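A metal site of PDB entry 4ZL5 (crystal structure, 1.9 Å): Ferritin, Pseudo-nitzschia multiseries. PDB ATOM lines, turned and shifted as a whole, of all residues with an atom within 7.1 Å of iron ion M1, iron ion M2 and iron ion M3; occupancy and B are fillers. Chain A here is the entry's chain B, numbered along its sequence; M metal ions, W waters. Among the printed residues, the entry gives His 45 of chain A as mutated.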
ATOM      1  N   GLN A  12     -17.804  11.351 -20.340  1.00  0.00           N
ATOM      2  CA  GLN A  12     -17.405  12.749 -20.218  1.00  0.00           C
ATOM      3  C   GLN A  12     -17.432  13.421 -21.563  1.00  0.00           C
ATOM      4  O   GLN A  12     -17.778  14.572 -21.666  1.00  0.00           O
ATOM      5  CB  GLN A  12     -16.009  12.860 -19.639  1.00  0.00           C
ATOM      6  CG  GLN A  12     -15.604  14.269 -19.311  1.00  0.00           C
ATOM      7  CD  GLN A  12     -16.501  14.896 -18.245  1.00  0.00           C
ATOM      8  OE1 GLN A  12     -17.018  14.189 -17.363  1.00  0.00           O
ATOM      9  NE2 GLN A  12     -16.698  16.177 -18.337  1.00  0.00           N
ATOM     10  N   GLN A  15     -20.920  14.273 -22.257  1.00  0.00           N
ATOM     11  CA  GLN A  15     -21.299  15.401 -21.456  1.00  0.00           C
ATOM     12  C   GLN A  15     -20.813  16.708 -22.102  1.00  0.00           C
ATOM     13  O   GLN A  15     -21.551  17.658 -22.073  1.00  0.00           O
ATOM     14  CB  GLN A  15     -20.760  15.251 -20.016  1.00  0.00           C
ATOM     15  CG  GLN A  15     -21.092  16.344 -19.037  1.00  0.00           C
ATOM     16  CD  GLN A  15     -22.612  16.514 -18.840  1.00  0.00           C
ATOM     17  OE1 GLN A  15     -23.356  15.494 -18.872  1.00  0.00           O
ATOM     18  NE2 GLN A  15     -23.097  17.802 -18.672  1.00  0.00           N
ATOM     19  N   GLU A  16     -19.586  16.728 -22.604  1.00  0.00           N
ATOM     20  CA  GLU A  16     -19.070  17.955 -23.217  1.00  0.00           C
ATOM     21  C   GLU A  16     -19.832  18.292 -24.472  1.00  0.00           C
ATOM     22  O   GLU A  16     -20.172  19.456 -24.662  1.00  0.00           O
ATOM     23  CB  GLU A  16     -17.589  17.805 -23.577  1.00  0.00           C
ATOM     24  CG  GLU A  16     -16.664  17.527 -22.423  1.00  0.00           C
ATOM     25  CD  GLU A  16     -16.674  18.658 -21.393  1.00  0.00           C
ATOM     26  OE1 GLU A  16     -17.000  19.794 -21.754  1.00  0.00           O
ATOM     27  OE2 GLU A  16     -16.399  18.362 -20.215  1.00  0.00           O
ATOM     28  N   ALA A  19     -23.267  19.516 -23.430  1.00  0.00           N
ATOM     29  CA  ALA A  19     -23.168  20.925 -23.030  1.00  0.00           C
ATOM     30  C   ALA A  19     -23.007  21.840 -24.226  1.00  0.00           C
ATOM     31  O   ALA A  19     -23.646  22.908 -24.250  1.00  0.00           O
ATOM     32  CB  ALA A  19     -22.030  21.141 -22.028  1.00  0.00           C
ATOM     33  N   TYR A  23     -25.522  24.994 -24.811  1.00  0.00           N
ATOM     34  CA  TYR A  23     -25.086  26.358 -25.036  1.00  0.00           C
ATOM     35  C   TYR A  23     -25.574  26.872 -26.366  1.00  0.00           C
ATOM     36  O   TYR A  23     -25.963  28.053 -26.483  1.00  0.00           O
ATOM     37  CB  TYR A  23     -23.555  26.448 -24.972  1.00  0.00           C
ATOM     38  CG  TYR A  23     -22.973  26.614 -23.609  1.00  0.00           C
ATOM     39  CD1 TYR A  23     -22.952  27.831 -22.980  1.00  0.00           C
ATOM     40  CD2 TYR A  23     -22.369  25.567 -22.941  1.00  0.00           C
ATOM     41  CE1 TYR A  23     -22.369  28.007 -21.736  1.00  0.00           C
ATOM     42  CE2 TYR A  23     -21.851  25.727 -21.649  1.00  0.00           C
ATOM     43  CZ  TYR A  23     -21.846  26.971 -21.087  1.00  0.00           C
ATOM     44  OH  TYR A  23     -21.283  27.263 -19.900  1.00  0.00           O
ATOM     45  N   HIS A  45     -19.092  29.773 -26.121  1.00  0.00           N
ATOM     46  CA  HIS A  45     -18.914  28.832 -25.118  1.00  0.00           C
ATOM     47  C   HIS A  45     -19.348  27.437 -25.689  1.00  0.00           C
ATOM     48  O   HIS A  45     -18.755  26.457 -25.337  1.00  0.00           O
ATOM     49  CB  HIS A  45     -19.658  29.212 -23.862  1.00  0.00           C
ATOM     50  CG  HIS A  45     -19.096  28.588 -22.638  1.00  0.00           C
ATOM     51  ND1 HIS A  45     -18.890  29.273 -21.460  1.00  0.00           N
ATOM     52  CD2 HIS A  45     -18.679  27.309 -22.390  1.00  0.00           C
ATOM     53  CE1 HIS A  45     -18.429  28.445 -20.533  1.00  0.00           C
ATOM     54  NE2 HIS A  45     -18.243  27.261 -21.088  1.00  0.00           N
ATOM     55  N   GLU A  48     -16.379  26.109 -27.334  1.00  0.00           N
ATOM     56  CA  GLU A  48     -15.384  25.743 -26.371  1.00  0.00           C
ATOM     57  C   GLU A  48     -15.709  24.401 -25.667  1.00  0.00           C
ATOM     58  O   GLU A  48     -14.781  23.573 -25.402  1.00  0.00           O
ATOM     59  CB  GLU A  48     -15.296  26.849 -25.312  1.00  0.00           C
ATOM     60  CG  GLU A  48     -14.551  26.410 -24.060  1.00  0.00           C
ATOM     61  CD  GLU A  48     -14.416  27.557 -23.062  1.00  0.00           C
ATOM     62  OE1 GLU A  48     -14.598  28.723 -23.475  1.00  0.00           O
ATOM     63  OE2 GLU A  48     -14.164  27.274 -21.864  1.00  0.00           O
ATOM     64  N   GLU A  49     -16.977  24.158 -25.400  1.00  0.00           N
ATOM     65  CA  GLU A  49     -17.317  22.791 -24.877  1.00  0.00           C
ATOM     66  C   GLU A  49     -16.979  21.684 -25.865  1.00  0.00           C
ATOM     67  O   GLU A  49     -16.544  20.582 -25.498  1.00  0.00           O
ATOM     68  CB  GLU A  49     -18.756  22.659 -24.571  1.00  0.00           C
ATOM     69  CG  GLU A  49     -19.279  23.554 -23.532  1.00  0.00           C
ATOM     70  CD  GLU A  49     -18.666  23.349 -22.162  1.00  0.00           C
ATOM     71  OE1 GLU A  49     -18.111  22.325 -21.791  1.00  0.00           O
ATOM     72  OE2 GLU A  49     -18.894  24.258 -21.449  1.00  0.00           O
ATOM     73  N   ARG A  50     -17.276  21.942 -27.137  1.00  0.00           N
ATOM     74  CA  ARG A  50     -16.928  21.003 -28.175  1.00  0.00           C
ATOM     75  C   ARG A  50     -15.413  20.786 -28.143  1.00  0.00           C
ATOM     76  O   ARG A  50     -14.919  19.648 -28.262  1.00  0.00           O
ATOM     77  CB  ARG A  50     -17.334  21.479 -29.562  1.00  0.00           C
ATOM     78  CG  ARG A  50     -17.048  20.424 -30.619  1.00  0.00           C
ATOM     79  CD  ARG A  50     -17.907  20.552 -31.892  1.00  0.00           C
ATOM     80  NE  ARG A  50     -17.494  19.586 -32.918  1.00  0.00           N
ATOM     81  CZ  ARG A  50     -16.412  19.780 -33.669  1.00  0.00           C
ATOM     82  NH1 ARG A  50     -15.661  20.837 -33.508  1.00  0.00           N
ATOM     83  NH2 ARG A  50     -15.992  18.848 -34.488  1.00  0.00           N
ATOM     84  N   HIS A  52     -13.393  20.969 -25.561  1.00  0.00           N
ATOM     85  CA  HIS A  52     -13.117  20.092 -24.434  1.00  0.00           C
ATOM     86  C   HIS A  52     -13.389  18.623 -24.789  1.00  0.00           C
ATOM     87  O   HIS A  52     -12.586  17.723 -24.477  1.00  0.00           O
ATOM     88  CB  HIS A  52     -13.937  20.415 -23.205  1.00  0.00           C
ATOM     89  CG  HIS A  52     -13.777  21.797 -22.703  1.00  0.00           C
ATOM     90  ND1 HIS A  52     -12.630  22.533 -22.919  1.00  0.00           N
ATOM     91  CD2 HIS A  52     -14.602  22.562 -21.950  1.00  0.00           C
ATOM     92  CE1 HIS A  52     -12.779  23.715 -22.359  1.00  0.00           C
ATOM     93  NE2 HIS A  52     -13.961  23.759 -21.764  1.00  0.00           N
ATOM     94  N   GLY A  53     -14.532  18.369 -25.389  1.00  0.00           N
ATOM     95  CA  GLY A  53     -14.796  17.006 -25.813  1.00  0.00           C
ATOM     96  C   GLY A  53     -13.724  16.446 -26.726  1.00  0.00           C
ATOM     97  O   GLY A  53     -13.326  15.290 -26.576  1.00  0.00           O
ATOM     98  N   PHE A  56     -10.670  15.381 -24.817  1.00  0.00           N
ATOM     99  CA  PHE A  56     -10.884  14.072 -24.260  1.00  0.00           C
ATOM    100  C   PHE A  56     -10.747  12.954 -25.235  1.00  0.00           C
ATOM    101  O   PHE A  56     -10.086  11.972 -24.923  1.00  0.00           O
ATOM    102  CB  PHE A  56     -12.205  13.969 -23.522  1.00  0.00           C
ATOM    103  CG  PHE A  56     -12.162  14.580 -22.108  1.00  0.00           C
ATOM    104  CD1 PHE A  56     -12.187  15.958 -21.934  1.00  0.00           C
ATOM    105  CD2 PHE A  56     -12.077  13.781 -20.991  1.00  0.00           C
ATOM    106  CE1 PHE A  56     -12.074  16.536 -20.674  1.00  0.00           C
ATOM    107  CE2 PHE A  56     -11.966  14.354 -19.715  1.00  0.00           C
ATOM    108  CZ  PHE A  56     -11.969  15.728 -19.565  1.00  0.00           C
ATOM    109  N   LEU A  94     -25.812  23.394 -15.729  1.00  0.00           N
ATOM    110  CA  LEU A  94     -25.080  22.595 -16.674  1.00  0.00           C
ATOM    111  C   LEU A  94     -23.588  22.469 -16.293  1.00  0.00           C
ATOM    112  O   LEU A  94     -22.995  21.380 -16.269  1.00  0.00           O
ATOM    113  CB  LEU A  94     -25.248  23.293 -18.022  1.00  0.00           C
ATOM    114  CG  LEU A  94     -24.493  22.680 -19.211  1.00  0.00           C
ATOM    115  CD1 LEU A  94     -25.098  21.367 -19.527  1.00  0.00           C
ATOM    116  CD2 LEU A  94     -24.545  23.560 -20.450  1.00  0.00           C
ATOM    117  N   GLU A  95     -22.985  23.612 -15.995  1.00  0.00           N
ATOM    118  CA  GLU A  95     -21.606  23.615 -15.556  1.00  0.00           C
ATOM    119  C   GLU A  95     -21.401  22.943 -14.244  1.00  0.00           C
ATOM    120  O   GLU A  95     -20.392  22.240 -14.064  1.00  0.00           O
ATOM    121  CB  GLU A  95     -21.032  25.021 -15.532  1.00  0.00           C
ATOM    122  CG  GLU A  95     -20.783  25.645 -16.919  1.00  0.00           C
ATOM    123  CD  GLU A  95     -19.733  24.975 -17.766  1.00  0.00           C
ATOM    124  OE1 GLU A  95     -19.015  24.039 -17.360  1.00  0.00           O
ATOM    125  OE2 GLU A  95     -19.585  25.474 -18.907  1.00  0.00           O
ATOM    126  N   ASN A  98     -21.268  19.472 -15.261  1.00  0.00           N
ATOM    127  CA  ASN A  98     -19.987  19.216 -15.954  1.00  0.00           C
ATOM    128  C   ASN A  98     -18.946  18.950 -14.801  1.00  0.00           C
ATOM    129  O   ASN A  98     -18.197  17.944 -14.810  1.00  0.00           O
ATOM    130  CB  ASN A  98     -19.451  20.373 -16.862  1.00  0.00           C
ATOM    131  CG  ASN A  98     -20.213  20.603 -18.230  1.00  0.00           C
ATOM    132  OD1 ASN A  98     -21.001  19.767 -18.716  1.00  0.00           O
ATOM    133  ND2 ASN A  98     -19.949  21.801 -18.853  1.00  0.00           N
ATOM    134  N   LEU A 102     -16.679  15.557 -13.938  1.00  0.00           N
ATOM    135  CA  LEU A 102     -15.189  15.494 -13.915  1.00  0.00           C
ATOM    136  C   LEU A 102     -14.665  14.960 -12.661  1.00  0.00           C
ATOM    137  O   LEU A 102     -13.632  14.291 -12.637  1.00  0.00           O
ATOM    138  CB  LEU A 102     -14.540  16.865 -14.058  1.00  0.00           C
ATOM    139  CG  LEU A 102     -14.523  17.417 -15.460  1.00  0.00           C
ATOM    140  CD1 LEU A 102     -14.013  18.853 -15.348  1.00  0.00           C
ATOM    141  CD2 LEU A 102     -13.617  16.624 -16.388  1.00  0.00           C
ATOM    142  N   PHE A 124      -8.541  20.882 -16.372  1.00  0.00           N
ATOM    143  CA  PHE A 124      -9.990  20.935 -16.441  1.00  0.00           C
ATOM    144  C   PHE A 124     -10.628  21.186 -15.061  1.00  0.00           C
ATOM    145  O   PHE A 124     -11.612  21.941 -14.965  1.00  0.00           O
ATOM    146  CB  PHE A 124     -10.549  19.653 -17.053  1.00  0.00           C
ATOM    147  CG  PHE A 124     -10.106  19.406 -18.468  1.00  0.00           C
ATOM    148  CD1 PHE A 124     -10.795  20.020 -19.535  1.00  0.00           C
ATOM    149  CD2 PHE A 124      -9.020  18.588 -18.760  1.00  0.00           C
ATOM    150  CE1 PHE A 124     -10.413  19.802 -20.839  1.00  0.00           C
ATOM    151  CE2 PHE A 124      -8.647  18.331 -20.078  1.00  0.00           C
ATOM    152  CZ  PHE A 124      -9.305  18.973 -21.113  1.00  0.00           C
ATOM    153  N   GLN A 127     -10.212  24.840 -14.693  1.00  0.00           N
ATOM    154  CA  GLN A 127     -11.046  25.608 -15.619  1.00  0.00           C
ATOM    155  C   GLN A 127     -12.497  25.636 -15.105  1.00  0.00           C
ATOM    156  O   GLN A 127     -13.147  26.704 -15.186  1.00  0.00           O
ATOM    157  CB  GLN A 127     -11.038  24.984 -17.006  1.00  0.00           C
ATOM    158  CG  GLN A 127     -12.056  25.652 -17.962  1.00  0.00           C
ATOM    159  CD  GLN A 127     -11.691  25.520 -19.435  1.00  0.00           C
ATOM    160  OE1 GLN A 127     -12.226  26.253 -20.286  1.00  0.00           O
ATOM    161  NE2 GLN A 127     -10.778  24.592 -19.759  1.00  0.00           N
ATOM    162  N   GLN A 128     -12.956  24.525 -14.557  1.00  0.00           N
ATOM    163  CA  GLN A 128     -14.340  24.398 -14.060  1.00  0.00           C
ATOM    164  C   GLN A 128     -14.528  25.393 -12.894  1.00  0.00           C
ATOM    165  O   GLN A 128     -15.580  26.068 -12.832  1.00  0.00           O
ATOM    166  CB  GLN A 128     -14.753  22.991 -13.638  1.00  0.00           C
ATOM    167  CG  GLN A 128     -15.078  22.079 -14.811  1.00  0.00           C
ATOM    168  CD  GLN A 128     -16.079  22.731 -15.757  1.00  0.00           C
ATOM    169  OE1 GLN A 128     -15.707  23.242 -16.836  1.00  0.00           O
ATOM    170  NE2 GLN A 128     -17.309  22.901 -15.268  1.00  0.00           N
ATOM    171  N   GLU A 131     -14.966  28.752 -14.573  1.00  0.00           N
ATOM    172  CA  GLU A 131     -16.259  28.847 -15.263  1.00  0.00           C
ATOM    173  C   GLU A 131     -17.428  28.996 -14.359  1.00  0.00           C
ATOM    174  O   GLU A 131     -18.256  29.859 -14.612  1.00  0.00           O
ATOM    175  CB  GLU A 131     -16.485  27.630 -16.197  1.00  0.00           C
ATOM    176  CG  GLU A 131     -15.545  27.786 -17.362  1.00  0.00           C
ATOM    177  CD  GLU A 131     -15.760  26.753 -18.481  1.00  0.00           C
ATOM    178  OE1 GLU A 131     -16.818  26.138 -18.453  1.00  0.00           O
ATOM    179  OE2 GLU A 131     -14.827  26.550 -19.291  1.00  0.00           O
ATOM    180  N   ILE A 135     -19.874  32.272 -14.500  1.00  0.00           N
ATOM    181  CA  ILE A 135     -21.302  32.154 -14.841  1.00  0.00           C
ATOM    182  C   ILE A 135     -22.164  32.515 -13.605  1.00  0.00           C
ATOM    183  O   ILE A 135     -23.212  33.141 -13.712  1.00  0.00           O
ATOM    184  CB  ILE A 135     -21.621  30.737 -15.356  1.00  0.00           C
ATOM    185  CG1 ILE A 135     -20.820  30.453 -16.617  1.00  0.00           C
ATOM    186  CG2 ILE A 135     -23.103  30.549 -15.568  1.00  0.00           C
ATOM    187  CD1 ILE A 135     -20.721  28.978 -16.917  1.00  0.00           C
HETATM  188 FE    FE M   1     -17.730  25.217 -20.024  1.00  0.00          FE
HETATM  189 FE    FE M   2     -14.223  25.123 -20.288  1.00  0.00          FE
HETATM  190 FE    FE M   3     -16.834  21.611 -20.477  1.00  0.00          FE
HETATM  191  O   HOH W   1     -17.100  23.367 -19.023  1.00  0.00           O
HETATM  192  O   HOH W   2     -15.322  20.595 -19.047  1.00  0.00           O
HETATM  193  O   HOH W   3     -16.180  25.449 -21.242  1.00  0.00           O
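Iron ion M2 is bound by the side-chain carboxylate (OE2) of Glu 131 (1.8 Å), a ring nitrogen (NE2) of His 52 (2.0 Å), water W3 (2.2 Å) and the side-chain amide oxygen (OE1) of Gln 127 (2.3 Å). Slightly farther from iron ion M2 lies OE2 of Glu 48 (2.7 Å).
OE1 of Glu 131 lies close to OE1 of Gln 128, 3.5 Å away. OE1 of Glu 95 is in hydrogen-bond range of ND2 of Asn 98. OH of Tyr 23 sits close to OE2 of Glu 95 (2.7 Å). The side-chain amide nitrogen (NE2) of Gln 128 sits at hydrogen-bond distance from the side-chain carboxylate (OE1) of Glu 95. The side-chain carboxylate (OE2) of Glu 16 sits at hydrogen-bond distance from the side-chain amide nitrogen (NE2) of Gln 12, at 2.9 Å. The side-chain amide oxygen of Gln 127 lies close to the side-chain carboxylate of Glu 48, 2.7 Å away. A ring nitrogen (ND1) of His 45 lies close to the side-chain hydroxyl (OH) of Tyr 23 (3.5 Å). OD1 of Asn 98 lies within hydrogen-bond range of NE2 of Gln 15 (2.9 Å).
Of the 21 residues printed, 4 come within 4 Å of iron ion M1. Along chain A the residues within 4 Å of iron ion M1 span positions 45 to 131. The nearest printed residue that does not touch iron ion M1 is Tyr 23 (4.1 Å).
Water W1 lies within hydrogen-bond range of OE1 of Gln 128 (2.6 Å), OE1 of Glu 95 (2.6 Å) and ND2 of Asn 98 (3.3 Å). Water W2 bridges the side-chain carboxylate of Glu 16 and the side-chain amide oxygen of Gln 128.
Merely in contact with iron ion M3: Asn 98. Four residues have an atom within 4 Å of iron ion M3: Glu 16, Glu 49, His 52 and Asn 98. The nearest printed residue that does not touch iron ion M3 is Gln 128 (4.1 Å).
The side-chain carboxylate (OE1) of Glu 49 binds iron ion M3 (2.0 Å). Iron ion M3 is bound by OE1 of Glu 16. Iron ion M3 is bound by water W1. Iron ion M3 is bound by water W2 (2.3 Å).
Iron ion M1 is bound by water W3, the side-chain carboxylate (OE1) of Glu 131, the side-chain carboxylate (OE2) of Glu 49, the side-chain carboxylate (OE2) of Glu 95, water W1 and a ring nitrogen (NE2) of His 45. Iron ion M1 has six donor atoms within binding distance.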
